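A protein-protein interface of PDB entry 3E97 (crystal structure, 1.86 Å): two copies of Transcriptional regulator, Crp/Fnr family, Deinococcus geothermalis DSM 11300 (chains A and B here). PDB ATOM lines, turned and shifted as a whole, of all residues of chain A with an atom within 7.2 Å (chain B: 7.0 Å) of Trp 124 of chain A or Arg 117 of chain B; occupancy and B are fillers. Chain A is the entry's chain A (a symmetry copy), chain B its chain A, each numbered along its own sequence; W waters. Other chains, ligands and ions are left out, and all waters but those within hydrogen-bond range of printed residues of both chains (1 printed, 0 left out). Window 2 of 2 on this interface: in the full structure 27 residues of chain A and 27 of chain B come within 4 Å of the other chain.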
ATOM      1  N   LEU A  13      10.521   7.752   6.291  1.00  0.00           N
ATOM      2  CA  LEU A  13      11.975   7.972   6.230  1.00  0.00           C
ATOM      3  C   LEU A  13      12.449   8.507   4.878  1.00  0.00           C
ATOM      4  O   LEU A  13      13.471   9.202   4.803  1.00  0.00           O
ATOM      5  CB  LEU A  13      12.755   6.699   6.569  1.00  0.00           C
ATOM      6  CG  LEU A  13      13.152   6.397   8.012  1.00  0.00           C
ATOM      7  CD1 LEU A  13      13.918   5.055   8.095  1.00  0.00           C
ATOM      8  CD2 LEU A  13      14.013   7.533   8.592  1.00  0.00           C
ATOM      9  N   LEU A 116      22.176   7.494   6.044  1.00  0.00           N
ATOM     10  CA  LEU A 116      21.990   8.745   6.775  1.00  0.00           C
ATOM     11  C   LEU A 116      23.165   9.706   6.550  1.00  0.00           C
ATOM     12  O   LEU A 116      22.956  10.886   6.330  1.00  0.00           O
ATOM     13  CB  LEU A 116      21.830   8.484   8.269  1.00  0.00           C
ATOM     14  CG  LEU A 116      20.513   7.837   8.723  1.00  0.00           C
ATOM     15  CD1 LEU A 116      20.606   7.489  10.194  1.00  0.00           C
ATOM     16  CD2 LEU A 116      19.298   8.737   8.420  1.00  0.00           C
ATOM     17  N   HIS A 119      23.041  10.791   2.681  1.00  0.00           N
ATOM     18  CA  HIS A 119      21.860  11.486   2.202  1.00  0.00           C
ATOM     19  C   HIS A 119      21.172  12.248   3.314  1.00  0.00           C
ATOM     20  O   HIS A 119      20.261  11.713   3.958  1.00  0.00           O
ATOM     21  CB  HIS A 119      20.886  10.478   1.580  1.00  0.00           C
ATOM     22  CG  HIS A 119      21.495   9.667   0.488  1.00  0.00           C
ATOM     23  ND1 HIS A 119      21.728  10.177  -0.776  1.00  0.00           N
ATOM     24  CD2 HIS A 119      21.932   8.385   0.466  1.00  0.00           C
ATOM     25  CE1 HIS A 119      22.281   9.238  -1.525  1.00  0.00           C
ATOM     26  NE2 HIS A 119      22.429   8.149  -0.790  1.00  0.00           N
ATOM     27  N   PRO A 120      21.594  13.510   3.532  1.00  0.00           N
ATOM     28  CA  PRO A 120      21.071  14.374   4.600  1.00  0.00           C
ATOM     29  C   PRO A 120      19.553  14.543   4.630  1.00  0.00           C
ATOM     30  O   PRO A 120      18.984  14.817   5.711  1.00  0.00           O
ATOM     31  CB  PRO A 120      21.760  15.724   4.333  1.00  0.00           C
ATOM     32  CG  PRO A 120      22.964  15.397   3.585  1.00  0.00           C
ATOM     33  CD  PRO A 120      22.630  14.206   2.747  1.00  0.00           C
ATOM     34  N   ARG A 121      18.881  14.408   3.487  1.00  0.00           N
ATOM     35  CA  ARG A 121      17.407  14.531   3.484  1.00  0.00           C
ATOM     36  C   ARG A 121      16.727  13.382   4.255  1.00  0.00           C
ATOM     37  O   ARG A 121      15.667  13.584   4.889  1.00  0.00           O
ATOM     38  CB  ARG A 121      16.862  14.696   2.067  1.00  0.00           C
ATOM     39  CG  ARG A 121      17.212  16.039   1.473  1.00  0.00           C
ATOM     40  CD  ARG A 121      16.763  16.182  -0.001  1.00  0.00           C
ATOM     41  N   VAL A 122      17.327  12.196   4.216  1.00  0.00           N
ATOM     42  CA  VAL A 122      16.813  11.043   4.961  1.00  0.00           C
ATOM     43  C   VAL A 122      17.032  11.323   6.469  1.00  0.00           C
ATOM     44  O   VAL A 122      16.167  11.035   7.308  1.00  0.00           O
ATOM     45  CB  VAL A 122      17.491   9.714   4.558  1.00  0.00           C
ATOM     46  CG1 VAL A 122      16.990   8.570   5.418  1.00  0.00           C
ATOM     47  CG2 VAL A 122      17.261   9.387   3.064  1.00  0.00           C
ATOM     48  N   LEU A 123      18.191  11.875   6.804  1.00  0.00           N
ATOM     49  CA  LEU A 123      18.506  12.235   8.195  1.00  0.00           C
ATOM     50  C   LEU A 123      17.566  13.321   8.720  1.00  0.00           C
ATOM     51  O   LEU A 123      17.151  13.289   9.891  1.00  0.00           O
ATOM     52  CB  LEU A 123      19.968  12.689   8.331  1.00  0.00           C
ATOM     53  CG  LEU A 123      20.388  13.113   9.745  1.00  0.00           C
ATOM     54  CD1 LEU A 123      20.237  11.960  10.752  1.00  0.00           C
ATOM     55  CD2 LEU A 123      21.791  13.623   9.700  1.00  0.00           C
ATOM     56  N   TRP A 124      17.227  14.289   7.874  1.00  0.00           N
ATOM     57  CA  TRP A 124      16.262  15.310   8.235  1.00  0.00           C
ATOM     58  C   TRP A 124      14.892  14.673   8.532  1.00  0.00           C
ATOM     59  O   TRP A 124      14.193  15.050   9.502  1.00  0.00           O
ATOM     60  CB  TRP A 124      16.105  16.345   7.123  1.00  0.00           C
ATOM     61  CG  TRP A 124      15.238  17.478   7.532  1.00  0.00           C
ATOM     62  CD1 TRP A 124      13.868  17.514   7.523  1.00  0.00           C
ATOM     63  CD2 TRP A 124      15.667  18.749   8.035  1.00  0.00           C
ATOM     64  NE1 TRP A 124      13.429  18.728   7.981  1.00  0.00           N
ATOM     65  CE2 TRP A 124      14.511  19.503   8.303  1.00  0.00           C
ATOM     66  CE3 TRP A 124      16.917  19.329   8.271  1.00  0.00           C
ATOM     67  CZ2 TRP A 124      14.571  20.802   8.800  1.00  0.00           C
ATOM     68  CZ3 TRP A 124      16.972  20.614   8.747  1.00  0.00           C
ATOM     69  CH2 TRP A 124      15.809  21.335   9.017  1.00  0.00           C
ATOM     70  N   ASN A 125      14.482  13.727   7.694  1.00  0.00           N
ATOM     71  CA  ASN A 125      13.213  13.016   7.942  1.00  0.00           C
ATOM     72  C   ASN A 125      13.231  12.298   9.293  1.00  0.00           C
ATOM     73  O   ASN A 125      12.247  12.352  10.042  1.00  0.00           O
ATOM     74  CB  ASN A 125      12.893  12.040   6.820  1.00  0.00           C
ATOM     75  CG  ASN A 125      12.434  12.742   5.554  1.00  0.00           C
ATOM     76  OD1 ASN A 125      11.944  13.873   5.598  1.00  0.00           O
ATOM     77  ND2 ASN A 125      12.568  12.066   4.426  1.00  0.00           N
ATOM     78  N   LEU A 126      14.328  11.626   9.599  1.00  0.00           N
ATOM     79  CA  LEU A 126      14.462  10.960  10.884  1.00  0.00           C
ATOM     80  C   LEU A 126      14.377  11.942  12.059  1.00  0.00           C
ATOM     81  O   LEU A 126      13.665  11.687  13.045  1.00  0.00           O
ATOM     82  CB  LEU A 126      15.758  10.157  10.918  1.00  0.00           C
ATOM     83  CG  LEU A 126      16.084   9.403  12.199  1.00  0.00           C
ATOM     84  CD1 LEU A 126      14.941   8.442  12.565  1.00  0.00           C
ATOM     85  CD2 LEU A 126      17.427   8.712  12.017  1.00  0.00           C
ATOM     86  N   ALA A 127      15.062  13.082  11.949  1.00  0.00           N
ATOM     87  CA  ALA A 127      15.052  14.081  13.029  1.00  0.00           C
ATOM     88  C   ALA A 127      13.632  14.613  13.275  1.00  0.00           C
ATOM     89  O   ALA A 127      13.196  14.789  14.438  1.00  0.00           O
ATOM     90  CB  ALA A 127      16.067  15.217  12.726  1.00  0.00           C
ATOM     91  N   GLU A 128      12.883  14.829  12.193  1.00  0.00           N
ATOM     92  CA  GLU A 128      11.495  15.279  12.302  1.00  0.00           C
ATOM     93  C   GLU A 128      10.622  14.255  13.007  1.00  0.00           C
ATOM     94  O   GLU A 128       9.783  14.616  13.866  1.00  0.00           O
ATOM     95  CB  GLU A 128      10.881  15.598  10.935  1.00  0.00           C
ATOM     96  CG  GLU A 128      11.405  16.843  10.268  1.00  0.00           C
ATOM     97  CD  GLU A 128      10.584  17.195   9.014  1.00  0.00           C
ATOM     98  OE1 GLU A 128      10.003  16.263   8.421  1.00  0.00           O
ATOM     99  OE2 GLU A 128      10.524  18.395   8.646  1.00  0.00           O
ATOM    100  N   MET A 129      10.789  12.996  12.626  1.00  0.00           N
ATOM    101  CA  MET A 129      10.046  11.888  13.238  1.00  0.00           C
ATOM    102  C   MET A 129      10.325  11.823  14.750  1.00  0.00           C
ATOM    103  O   MET A 129       9.385  11.752  15.555  1.00  0.00           O
ATOM    104  CB  MET A 129      10.426  10.571  12.558  1.00  0.00           C
ATOM    105  CG  MET A 129       9.946  10.501  11.112  1.00  0.00           C
ATOM    106  SD  MET A 129      10.883   9.097  10.107  1.00  0.00           S
ATOM    107  CE  MET A 129      10.819   7.811  11.418  1.00  0.00           C
ATOM    108  N   LEU A 130      11.606  11.903  15.114  1.00  0.00           N
ATOM    109  CA  LEU A 130      12.043  11.879  16.517  1.00  0.00           C
ATOM    110  C   LEU A 130      11.502  13.062  17.313  1.00  0.00           C
ATOM    111  O   LEU A 130      11.058  12.883  18.451  1.00  0.00           O
ATOM    112  CB  LEU A 130      13.574  11.816  16.590  1.00  0.00           C
ATOM    113  CG  LEU A 130      14.267  10.538  16.108  1.00  0.00           C
ATOM    114  CD1 LEU A 130      15.794  10.693  16.118  1.00  0.00           C
ATOM    115  CD2 LEU A 130      13.880   9.335  16.949  1.00  0.00           C
ATOM    116  N   ARG A 132       8.752  14.837  16.624  1.00  0.00           N
ATOM    117  CA  ARG A 132       7.335  14.556  16.824  1.00  0.00           C
ATOM    118  C   ARG A 132       7.089  13.543  17.927  1.00  0.00           C
ATOM    119  O   ARG A 132       6.121  13.691  18.683  1.00  0.00           O
ATOM    120  CB  ARG A 132       6.682  14.110  15.514  1.00  0.00           C
ATOM    121  CG  ARG A 132       6.617  15.233  14.466  1.00  0.00           C
ATOM    122  CD  ARG A 132       5.692  14.867  13.303  1.00  0.00           C
ATOM    123  NE  ARG A 132       6.058  13.634  12.604  1.00  0.00           N
ATOM    124  CZ  ARG A 132       6.846  13.559  11.519  1.00  0.00           C
ATOM    125  NH1 ARG A 132       7.397  14.639  10.979  1.00  0.00           N
ATOM    126  NH2 ARG A 132       7.100  12.382  10.968  1.00  0.00           N
ATOM    127  N   VAL B  86      12.384  23.338  15.408  1.00  0.00           N
ATOM    128  CA  VAL B  86      12.823  23.504  14.027  1.00  0.00           C
ATOM    129  C   VAL B  86      12.436  22.253  13.199  1.00  0.00           C
ATOM    130  O   VAL B  86      12.420  22.298  11.960  1.00  0.00           O
ATOM    131  CB  VAL B  86      14.346  23.746  13.980  1.00  0.00           C
ATOM    132  CG1 VAL B  86      14.852  23.861  12.559  1.00  0.00           C
ATOM    133  CG2 VAL B  86      14.682  25.006  14.777  1.00  0.00           C
ATOM    134  N   LEU B  87      12.105  21.163  13.901  1.00  0.00           N
ATOM    135  CA  LEU B  87      11.774  19.869  13.291  1.00  0.00           C
ATOM    136  C   LEU B  87      10.309  19.466  13.470  1.00  0.00           C
ATOM    137  O   LEU B  87       9.725  18.829  12.603  1.00  0.00           O
ATOM    138  CB  LEU B  87      12.674  18.800  13.895  1.00  0.00           C
ATOM    139  CG  LEU B  87      14.157  18.928  13.596  1.00  0.00           C
ATOM    140  CD1 LEU B  87      14.920  17.973  14.481  1.00  0.00           C
ATOM    141  CD2 LEU B  87      14.435  18.647  12.135  1.00  0.00           C
ATOM    142  N   PHE B 112      18.866  28.632  12.544  1.00  0.00           N
ATOM    143  CA  PHE B 112      19.177  27.267  12.976  1.00  0.00           C
ATOM    144  C   PHE B 112      18.874  26.278  11.845  1.00  0.00           C
ATOM    145  O   PHE B 112      19.629  25.345  11.618  1.00  0.00           O
ATOM    146  CB  PHE B 112      18.386  26.930  14.248  1.00  0.00           C
ATOM    147  CG  PHE B 112      18.681  25.567  14.837  1.00  0.00           C
ATOM    148  CD1 PHE B 112      19.976  25.097  14.971  1.00  0.00           C
ATOM    149  CD2 PHE B 112      17.656  24.804  15.339  1.00  0.00           C
ATOM    150  CE1 PHE B 112      20.229  23.865  15.548  1.00  0.00           C
ATOM    151  CE2 PHE B 112      17.900  23.559  15.932  1.00  0.00           C
ATOM    152  CZ  PHE B 112      19.178  23.099  16.041  1.00  0.00           C
ATOM    153  N   GLU B 113      17.785  26.517  11.121  1.00  0.00           N
ATOM    154  CA  GLU B 113      17.408  25.680   9.978  1.00  0.00           C
ATOM    155  C   GLU B 113      18.518  25.729   8.908  1.00  0.00           C
ATOM    156  O   GLU B 113      18.948  24.705   8.392  1.00  0.00           O
ATOM    157  CB  GLU B 113      16.042  26.127   9.421  1.00  0.00           C
ATOM    158  CG  GLU B 113      14.865  25.838  10.382  1.00  0.00           C
ATOM    159  CD  GLU B 113      13.527  26.548  10.055  1.00  0.00           C
ATOM    160  OE1 GLU B 113      13.515  27.716   9.589  1.00  0.00           O
ATOM    161  OE2 GLU B 113      12.472  25.938  10.326  1.00  0.00           O
ATOM    162  N   LEU B 114      19.022  26.919   8.627  1.00  0.00           N
ATOM    163  CA  LEU B 114      20.084  27.073   7.638  1.00  0.00           C
ATOM    164  C   LEU B 114      21.343  26.291   8.018  1.00  0.00           C
ATOM    165  O   LEU B 114      21.950  25.627   7.168  1.00  0.00           O
ATOM    166  CB  LEU B 114      20.430  28.564   7.465  1.00  0.00           C
ATOM    167  CG  LEU B 114      21.479  28.957   6.417  1.00  0.00           C
ATOM    168  CD1 LEU B 114      21.153  28.347   5.039  1.00  0.00           C
ATOM    169  CD2 LEU B 114      21.595  30.486   6.327  1.00  0.00           C
ATOM    170  N   ILE B 115      21.729  26.382   9.292  1.00  0.00           N
ATOM    171  CA  ILE B 115      22.923  25.702   9.790  1.00  0.00           C
ATOM    172  C   ILE B 115      22.747  24.191   9.671  1.00  0.00           C
ATOM    173  O   ILE B 115      23.674  23.487   9.275  1.00  0.00           O
ATOM    174  CB  ILE B 115      23.233  26.105  11.257  1.00  0.00           C
ATOM    175  CG1 ILE B 115      23.584  27.598  11.342  1.00  0.00           C
ATOM    176  CG2 ILE B 115      24.400  25.284  11.821  1.00  0.00           C
ATOM    177  CD1 ILE B 115      23.623  28.139  12.761  1.00  0.00           C
ATOM    178  N   LEU B 116      21.549  23.703  10.005  1.00  0.00           N
ATOM    179  CA  LEU B 116      21.252  22.275   9.922  1.00  0.00           C
ATOM    180  C   LEU B 116      21.321  21.771   8.474  1.00  0.00           C
ATOM    181  O   LEU B 116      21.883  20.721   8.220  1.00  0.00           O
ATOM    182  CB  LEU B 116      19.873  21.971  10.498  1.00  0.00           C
ATOM    183  CG  LEU B 116      19.720  22.078  12.023  1.00  0.00           C
ATOM    184  CD1 LEU B 116      18.258  21.923  12.391  1.00  0.00           C
ATOM    185  CD2 LEU B 116      20.610  21.058  12.761  1.00  0.00           C
ATOM    186  N   ARG B 117      20.753  22.534   7.548  1.00  0.00           N
ATOM    187  CA  ARG B 117      20.776  22.165   6.116  1.00  0.00           C
ATOM    188  C   ARG B 117      22.192  22.197   5.534  1.00  0.00           C
ATOM    189  O   ARG B 117      22.560  21.334   4.747  1.00  0.00           O
ATOM    190  CB  ARG B 117      19.890  23.110   5.292  1.00  0.00           C
ATOM    191  CG  ARG B 117      18.408  23.100   5.629  1.00  0.00           C
ATOM    192  CD  ARG B 117      17.725  21.808   5.236  1.00  0.00           C
ATOM    193  NE  ARG B 117      16.264  21.903   5.348  1.00  0.00           N
ATOM    194  CZ  ARG B 117      15.415  20.913   5.067  1.00  0.00           C
ATOM    195  NH1 ARG B 117      15.864  19.726   4.660  1.00  0.00           N
ATOM    196  NH2 ARG B 117      14.109  21.105   5.201  1.00  0.00           N
ATOM    197  N   ARG B 118      22.984  23.190   5.925  1.00  0.00           N
ATOM    198  CA  ARG B 118      24.343  23.348   5.431  1.00  0.00           C
ATOM    199  C   ARG B 118      25.387  22.453   6.083  1.00  0.00           C
ATOM    200  O   ARG B 118      26.402  22.148   5.457  1.00  0.00           O
ATOM    201  CB  ARG B 118      24.804  24.802   5.606  1.00  0.00           C
ATOM    202  CG  ARG B 118      24.133  25.800   4.674  1.00  0.00           C
ATOM    203  CD  ARG B 118      24.600  27.234   4.939  1.00  0.00           C
ATOM    204  NE  ARG B 118      26.061  27.378   4.943  1.00  0.00           N
ATOM    205  CZ  ARG B 118      26.823  27.676   3.885  1.00  0.00           C
ATOM    206  NH1 ARG B 118      26.297  27.865   2.678  1.00  0.00           N
ATOM    207  NH2 ARG B 118      28.143  27.776   4.037  1.00  0.00           N
ATOM    208  N   HIS B 119      25.167  22.054   7.338  1.00  0.00           N
ATOM    209  CA  HIS B 119      26.157  21.288   8.075  1.00  0.00           C
ATOM    210  C   HIS B 119      25.551  20.051   8.701  1.00  0.00           C
ATOM    211  O   HIS B 119      25.121  20.093   9.861  1.00  0.00           O
ATOM    212  CB  HIS B 119      26.786  22.170   9.161  1.00  0.00           C
ATOM    213  CG  HIS B 119      27.386  23.425   8.626  1.00  0.00           C
ATOM    214  ND1 HIS B 119      28.594  23.444   7.953  1.00  0.00           N
ATOM    215  CD2 HIS B 119      26.946  24.705   8.653  1.00  0.00           C
ATOM    216  CE1 HIS B 119      28.866  24.686   7.592  1.00  0.00           C
ATOM    217  NE2 HIS B 119      27.876  25.466   7.990  1.00  0.00           N
ATOM    218  N   PRO B 120      25.531  18.937   7.942  1.00  0.00           N
ATOM    219  CA  PRO B 120      24.939  17.663   8.375  1.00  0.00           C
ATOM    220  C   PRO B 120      25.440  17.120   9.712  1.00  0.00           C
ATOM    221  O   PRO B 120      24.704  16.367  10.388  1.00  0.00           O
ATOM    222  CB  PRO B 120      25.299  16.698   7.231  1.00  0.00           C
ATOM    223  CG  PRO B 120      25.516  17.547   6.070  1.00  0.00           C
ATOM    224  CD  PRO B 120      26.091  18.827   6.583  1.00  0.00           C
ATOM    225  N   LEU B 123      23.225  18.475  12.350  1.00  0.00           N
ATOM    226  CA  LEU B 123      21.942  17.759  12.260  1.00  0.00           C
ATOM    227  C   LEU B 123      22.035  16.362  12.874  1.00  0.00           C
ATOM    228  O   LEU B 123      21.090  15.895  13.532  1.00  0.00           O
ATOM    229  CB  LEU B 123      21.463  17.666  10.802  1.00  0.00           C
ATOM    230  CG  LEU B 123      20.142  16.911  10.599  1.00  0.00           C
ATOM    231  CD1 LEU B 123      18.982  17.582  11.355  1.00  0.00           C
ATOM    232  CD2 LEU B 123      19.861  16.813   9.136  1.00  0.00           C
ATOM    233  N   LEU B 126      21.848  16.798  16.603  1.00  0.00           N
ATOM    234  CA  LEU B 126      20.464  17.005  16.998  1.00  0.00           C
ATOM    235  C   LEU B 126      19.662  15.698  17.015  1.00  0.00           C
ATOM    236  O   LEU B 126      18.926  15.421  17.977  1.00  0.00           O
ATOM    237  CB  LEU B 126      19.817  18.046  16.092  1.00  0.00           C
ATOM    238  CG  LEU B 126      18.354  18.383  16.340  1.00  0.00           C
ATOM    239  CD1 LEU B 126      18.146  18.847  17.790  1.00  0.00           C
ATOM    240  CD2 LEU B 126      17.917  19.407  15.303  1.00  0.00           C
HETATM  241  O   HOH W   1       7.489  17.466  11.819  1.00  0.00           O
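Printed residues of chain A that touch a printed residue of chain B: Leu 123, Trp 124, Ala 127 and Glu 128. Hydrophobic or aromatic side chains of chain A within 4 Å of the printed part of chain B: Leu 123, Trp 124 and Ala 127. Along chain A the printed residues that touch a printed residue of chain B span positions 123 to 128. Printed residues of chain B that touch a printed residue of chain A: Leu 87, Leu 116, Arg 117 and Leu 123.
Arg 117 of chain B touches just one residue of chain A: Trp 124. Printed residues of chain A within 4 Å of Leu 116 of chain B: Trp 124. Printed residues of chain B within 4 Å of Leu 123 of chain A: Leu 123 (3.8 Å). The nearest residue of chain A that does not touch Arg 117 of chain B is Arg 121 of chain A (5.1 Å). The nearest printed residue of chain B that does not touch Leu 123 of chain A is Pro 120 of chain B (4.1 Å).
OE2 of Glu 128 of chain A lies within hydrogen-bond range of NE1 of Trp 124 of chain A (3.0 Å). OE1 of Glu 128 of chain A lies within salt-bridge range of NH1 of Arg 132 of chain A, 3.996 Å away.
Water W1 lies within hydrogen-bond range of O of Leu 87 of chain B (2.7 Å) and NH1 of Arg 132 of chain A (3.0 Å).
Leu 123 of chain B touches its own counterpart, Leu 123 of chain A. Of the 8 pairs that touch across the chains among the printed residues, 1 has its exchanged pair printed and touching as well.
Among the printed residues, pairs that only touch across the chains: Ala 127 of chain A with Leu 87 of chain B (3.5 Å), Glu 128 of chain A with Leu 87 of chain B (3.5 Å), Trp 124 of chain A with Arg 117 of chain B (3.5 Å), Trp 124 of chain A with Leu 116 of chain B (3.7 Å), Leu 123 of chain A with Leu 123 of chain B (3.8 Å), Trp 124 of chain A with Leu 123 of chain B (3.9 Å), Trp 124 of chain A with Leu 87 of chain B (3.9 Å) and Ala 127 of chain A with Leu 123 of chain B (3.996 Å).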
